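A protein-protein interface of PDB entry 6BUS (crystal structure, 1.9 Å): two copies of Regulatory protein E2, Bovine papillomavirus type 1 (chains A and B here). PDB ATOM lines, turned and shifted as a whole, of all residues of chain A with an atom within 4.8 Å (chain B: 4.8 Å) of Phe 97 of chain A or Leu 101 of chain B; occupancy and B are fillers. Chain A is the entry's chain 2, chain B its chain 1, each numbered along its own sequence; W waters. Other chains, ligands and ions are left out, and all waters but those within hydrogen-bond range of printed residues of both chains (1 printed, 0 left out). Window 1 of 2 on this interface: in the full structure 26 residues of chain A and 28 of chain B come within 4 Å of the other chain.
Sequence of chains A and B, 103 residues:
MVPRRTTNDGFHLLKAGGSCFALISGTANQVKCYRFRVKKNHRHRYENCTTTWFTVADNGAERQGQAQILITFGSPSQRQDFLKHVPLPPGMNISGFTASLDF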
ATOM      1  N   SER A  19       1.981   8.189 -10.873  1.00  0.00           N
ATOM      2  CA  SER A  19       1.543   9.333 -10.083  1.00  0.00           C
ATOM      3  C   SER A  19       1.992   9.206  -8.632  1.00  0.00           C
ATOM      4  O   SER A  19       2.425   8.138  -8.197  1.00  0.00           O
ATOM      5  CB  SER A  19       0.022   9.481 -10.152  1.00  0.00           C
ATOM      6  OG  SER A  19      -0.404   9.757 -11.475  1.00  0.00           O
ATOM      7  N   CYS A  20       1.887  10.301  -7.886  1.00  0.00           N
ATOM      8  CA  CYS A  20       2.277  10.313  -6.498  1.00  0.00           C
ATOM      9  C   CYS A  20       1.360  11.091  -5.576  1.00  0.00           C
ATOM     10  O   CYS A  20       0.606  12.001  -5.950  1.00  0.00           O
ATOM     11  CB  CYS A  20       3.765  10.657  -6.322  1.00  0.00           C
ATOM     12  SG  CYS A  20       4.144  12.386  -6.456  1.00  0.00           S
ATOM     13  N   PHE A  21       1.379  10.648  -4.340  1.00  0.00           N
ATOM     14  CA  PHE A  21       0.472  11.192  -3.347  1.00  0.00           C
ATOM     15  C   PHE A  21       1.104  11.055  -1.983  1.00  0.00           C
ATOM     16  O   PHE A  21       2.251  10.573  -1.825  1.00  0.00           O
ATOM     17  CB  PHE A  21      -0.941  10.543  -3.431  1.00  0.00           C
ATOM     18  CG  PHE A  21      -0.980   9.054  -3.063  1.00  0.00           C
ATOM     19  CD1 PHE A  21      -0.722   8.060  -4.035  1.00  0.00           C
ATOM     20  CD2 PHE A  21      -1.308   8.661  -1.779  1.00  0.00           C
ATOM     21  CE1 PHE A  21      -0.764   6.691  -3.689  1.00  0.00           C
ATOM     22  CE2 PHE A  21      -1.333   7.310  -1.409  1.00  0.00           C
ATOM     23  CZ  PHE A  21      -1.073   6.316  -2.368  1.00  0.00           C
ATOM     24  N   ALA A  22       0.363  11.558  -1.016  1.00  0.00           N
ATOM     25  CA  ALA A  22       0.705  11.524   0.372  1.00  0.00           C
ATOM     26  C   ALA A  22      -0.588  11.295   1.228  1.00  0.00           C
ATOM     27  O   ALA A  22      -1.699  11.722   0.842  1.00  0.00           O
ATOM     28  CB  ALA A  22       1.357  12.856   0.717  1.00  0.00           C
ATOM     29  N   LEU A  23      -0.381  10.612   2.365  1.00  0.00           N
ATOM     30  CA  LEU A  23      -1.367  10.358   3.398  1.00  0.00           C
ATOM     31  C   LEU A  23      -1.027  11.196   4.616  1.00  0.00           C
ATOM     32  O   LEU A  23       0.024  11.043   5.187  1.00  0.00           O
ATOM     33  CB  LEU A  23      -1.302   8.859   3.739  1.00  0.00           C
ATOM     34  CG  LEU A  23      -2.172   8.193   4.787  1.00  0.00           C
ATOM     35  CD1 LEU A  23      -3.632   8.522   4.532  1.00  0.00           C
ATOM     36  CD2 LEU A  23      -1.985   6.659   4.787  1.00  0.00           C
ATOM     37  N   ARG A  79       5.326  17.407  -5.673  1.00  0.00           N
ATOM     38  CA  ARG A  79       5.356  16.899  -4.324  1.00  0.00           C
ATOM     39  C   ARG A  79       6.597  17.357  -3.574  1.00  0.00           C
ATOM     40  O   ARG A  79       6.509  17.686  -2.403  1.00  0.00           O
ATOM     41  CB  ARG A  79       5.260  15.379  -4.275  1.00  0.00           C
ATOM     42  CG  ARG A  79       5.337  14.820  -2.872  1.00  0.00           C
ATOM     43  CD  ARG A  79       5.138  13.304  -2.754  1.00  0.00           C
ATOM     44  NE  ARG A  79       6.208  12.526  -3.404  1.00  0.00           N
ATOM     45  CZ  ARG A  79       6.223  11.189  -3.447  1.00  0.00           C
ATOM     46  NH1 ARG A  79       5.257  10.469  -2.915  1.00  0.00           N
ATOM     47  NH2 ARG A  79       7.205  10.543  -4.072  1.00  0.00           N
ATOM     48  N   SER A  95       3.006  10.224   5.109  1.00  0.00           N
ATOM     49  CA  SER A  95       3.734   9.204   4.367  1.00  0.00           C
ATOM     50  C   SER A  95       3.510   9.546   2.937  1.00  0.00           C
ATOM     51  O   SER A  95       2.448  10.017   2.605  1.00  0.00           O
ATOM     52  CB  SER A  95       3.150   7.812   4.565  1.00  0.00           C
ATOM     53  OG  SER A  95       3.169   7.374   5.861  1.00  0.00           O
ATOM     54  N   GLY A  96       4.465   9.257   2.084  1.00  0.00           N
ATOM     55  CA  GLY A  96       4.353   9.517   0.652  1.00  0.00           C
ATOM     56  C   GLY A  96       4.396   8.193  -0.107  1.00  0.00           C
ATOM     57  O   GLY A  96       5.074   7.256   0.307  1.00  0.00           O
ATOM     58  N   PHE A  97       3.676   8.130  -1.205  1.00  0.00           N
ATOM     59  CA  PHE A  97       3.501   6.895  -2.012  1.00  0.00           C
ATOM     60  C   PHE A  97       3.444   7.291  -3.452  1.00  0.00           C
ATOM     61  O   PHE A  97       3.209   8.451  -3.797  1.00  0.00           O
ATOM     62  CB  PHE A  97       2.188   6.189  -1.696  1.00  0.00           C
ATOM     63  CG  PHE A  97       2.009   5.855  -0.246  1.00  0.00           C
ATOM     64  CD1 PHE A  97       1.445   6.787   0.612  1.00  0.00           C
ATOM     65  CD2 PHE A  97       2.389   4.630   0.235  1.00  0.00           C
ATOM     66  CE1 PHE A  97       1.265   6.489   1.957  1.00  0.00           C
ATOM     67  CE2 PHE A  97       2.210   4.293   1.554  1.00  0.00           C
ATOM     68  CZ  PHE A  97       1.642   5.247   2.439  1.00  0.00           C
ATOM     69  N   THR A  98       3.731   6.324  -4.297  1.00  0.00           N
ATOM     70  CA  THR A  98       3.536   6.399  -5.753  1.00  0.00           C
ATOM     71  C   THR A  98       2.759   5.145  -6.108  1.00  0.00           C
ATOM     72  O   THR A  98       3.120   4.058  -5.627  1.00  0.00           O
ATOM     73  CB  THR A  98       4.882   6.324  -6.492  1.00  0.00           C
ATOM     74  OG1 THR A  98       5.673   7.468  -6.128  1.00  0.00           O
ATOM     75  CG2 THR A  98       4.675   6.272  -7.958  1.00  0.00           C
ATOM     76  N   ALA A  99       1.682   5.324  -6.878  1.00  0.00           N
ATOM     77  CA  ALA A  99       0.813   4.243  -7.320  1.00  0.00           C
ATOM     78  C   ALA A  99       0.802   4.036  -8.816  1.00  0.00           C
ATOM     79  O   ALA A  99       0.765   4.972  -9.598  1.00  0.00           O
ATOM     80  CB  ALA A  99      -0.605   4.484  -6.823  1.00  0.00           C
ATOM     81  N   ALA B  99       0.903   0.538  -4.811  1.00  0.00           N
ATOM     82  CA  ALA B  99       1.597   1.712  -4.294  1.00  0.00           C
ATOM     83  C   ALA B  99       2.910   1.344  -3.625  1.00  0.00           C
ATOM     84  O   ALA B  99       2.914   0.493  -2.719  1.00  0.00           O
ATOM     85  CB  ALA B  99       0.734   2.453  -3.280  1.00  0.00           C
ATOM     86  N   SER B 100       3.989   2.015  -4.008  1.00  0.00           N
ATOM     87  CA  SER B 100       5.243   1.904  -3.268  1.00  0.00           C
ATOM     88  C   SER B 100       5.207   2.853  -2.107  1.00  0.00           C
ATOM     89  O   SER B 100       4.599   3.943  -2.213  1.00  0.00           O
ATOM     90  CB  SER B 100       6.446   2.269  -4.165  1.00  0.00           C
ATOM     91  OG  SER B 100       6.228   3.582  -4.740  1.00  0.00           O
ATOM     92  N   LEU B 101       5.871   2.511  -1.016  1.00  0.00           N
ATOM     93  CA  LEU B 101       6.118   3.512   0.006  1.00  0.00           C
ATOM     94  C   LEU B 101       7.373   4.352  -0.350  1.00  0.00           C
ATOM     95  O   LEU B 101       8.469   3.796  -0.545  1.00  0.00           O
ATOM     96  CB  LEU B 101       6.249   2.843   1.360  1.00  0.00           C
ATOM     97  CG  LEU B 101       6.473   3.644   2.672  1.00  0.00           C
ATOM     98  CD1 LEU B 101       7.759   4.419   2.641  1.00  0.00           C
ATOM     99  CD2 LEU B 101       5.357   4.572   3.023  1.00  0.00           C
ATOM    100  N   ASP B 102       7.214   5.688  -0.416  1.00  0.00           N
ATOM    101  CA  ASP B 102       8.324   6.611  -0.717  1.00  0.00           C
ATOM    102  C   ASP B 102       9.006   7.260   0.519  1.00  0.00           C
ATOM    103  O   ASP B 102      10.249   7.482   0.503  1.00  0.00           O
ATOM    104  CB  ASP B 102       7.845   7.685  -1.711  1.00  0.00           C
ATOM    105  CG  ASP B 102       7.348   7.100  -3.028  1.00  0.00           C
ATOM    106  OD1 ASP B 102       7.797   6.006  -3.405  1.00  0.00           O
ATOM    107  OD2 ASP B 102       6.535   7.724  -3.751  1.00  0.00           O
ATOM    108  N   PHE B 103       8.208   7.602   1.554  1.00  0.00           N
ATOM    109  CA  PHE B 103       8.737   8.124   2.833  1.00  0.00           C
ATOM    110  C   PHE B 103       7.689   8.050   3.931  1.00  0.00           C
ATOM    111  O   PHE B 103       8.064   8.140   5.140  1.00  0.00           O
ATOM    112  CB  PHE B 103       9.212   9.569   2.710  1.00  0.00           C
ATOM    113  CG  PHE B 103       8.179  10.518   2.126  1.00  0.00           C
ATOM    114  CD1 PHE B 103       7.277  11.163   2.929  1.00  0.00           C
ATOM    115  CD2 PHE B 103       8.136  10.756   0.765  1.00  0.00           C
ATOM    116  CE1 PHE B 103       6.381  12.041   2.383  1.00  0.00           C
ATOM    117  CE2 PHE B 103       7.247  11.607   0.227  1.00  0.00           C
ATOM    118  CZ  PHE B 103       6.369  12.258   1.029  1.00  0.00           C
ATOM    119  OXT PHE B 103       6.485   7.785   3.630  1.00  0.00           O
HETATM  120  O   HOH W   1       6.159   7.150   6.616  1.00  0.00           O
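Among the printed residues, merely in contact across the chains: Thr 98 of chain A with Ala 99 of chain B (3.1 Å), Phe 97 of chain A with Ser 100 of chain B (3.2 Å), Ser 95 of chain A with Phe 103 of chain B (3.2 Å), Phe 97 of chain A with Leu 101 of chain B (3.5 Å), Gly 96 of chain A with Leu 101 of chain B (3.8 Å) and Arg 79 of chain A with Phe 103 of chain B (3.8 Å).
Of the printed residues of chain B, Phe 97 of chain A touches Ser 100 (3.2 Å), Leu 101 (3.5 Å) and Asp 102 (3.1 Å).
Leu 101 of chain B touches just these residues of chain A: Gly 96 and Phe 97.
Printed residues of chain B within 4 Å of Arg 79 of chain A: Asp 102 and Phe 103.
Of the printed residues of chain B, Gly 96 of chain A touches Leu 101, Asp 102 and Phe 103.
Of the printed residues of chain B, Thr 98 of chain A touches Ala 99 (3.1 Å), Ser 100 (2.7 Å) and Asp 102 (2.5 Å).
The nearest printed residue of chain A that does not touch Phe 103 of chain B is Ala 22 of chain A (5.1 Å).
The backbone NH of Ser 100 of chain B lies within hydrogen-bond range of the backbone carbonyl oxygen of Thr 98 of chain A (2.7 Å).
The side-chain carboxylate (OD2) of Asp 102 of chain B lies within salt-bridge range of the guanidinium group (NH2) of Arg 79 of chain A.
The backbone NH of Asp 102 of chain B sits at hydrogen-bond distance from the backbone carbonyl oxygen of Gly 96 of chain A, 2.7 Å away.
OD2 of Asp 102 of chain B is in hydrogen-bond range of OG1 of Thr 98 of chain A (2.5 Å).
The chain-end carboxylate of Phe 103 of chain B sits at hydrogen-bond distance from the backbone NH of Gly 96 of chain A (2.9 Å).
The backbone carbonyl oxygen (O) of Phe 97 of chain A sits close to the side-chain carboxylate (OD2) of Asp 102 of chain B (3.4 Å).
The side-chain hydroxyl of Ser 100 of chain B sits at hydrogen-bond distance from the side-chain carboxylate of Asp 102 of chain B (3.2 Å).
The side-chain sulfur (SG) of Cys 20 of chain A lies within hydrogen-bond range of the guanidinium group (NE) of Arg 79 of chain A.
The guanidinium group (NH1) of Arg 79 of chain A lies within hydrogen-bond range of the backbone carbonyl oxygen (O) of Phe 21 of chain A, at 3.2 Å.
O of Phe 21 of chain A is in hydrogen-bond range of N of Phe 97 of chain A (2.9 Å).
The backbone NH of Leu 23 of chain A is in hydrogen-bond range of the backbone carbonyl oxygen of Ser 95 of chain A (2.9 Å).
NH1 of Arg 79 of chain A sits at hydrogen-bond distance from O of Phe 97 of chain A (3.0 Å).
Water W1 bridges the chain-end carboxylate (O) of Phe 103 of chain B (2.6 Å) and the side-chain hydroxyl (OG) of Ser 95 of chain A (3.1 Å).
Position printed for both chains: 99.
Hydrophobic or aromatic side chains of chain B that line the printed part of chain A: Ala 99, Leu 101 and Phe 103.
Among the printed residues, Asp or Glu carboxylates within 4 Å of a Lys or Arg side-chain nitrogen of the other chain: Arg 79 of chain A with Asp 102 of chain B.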
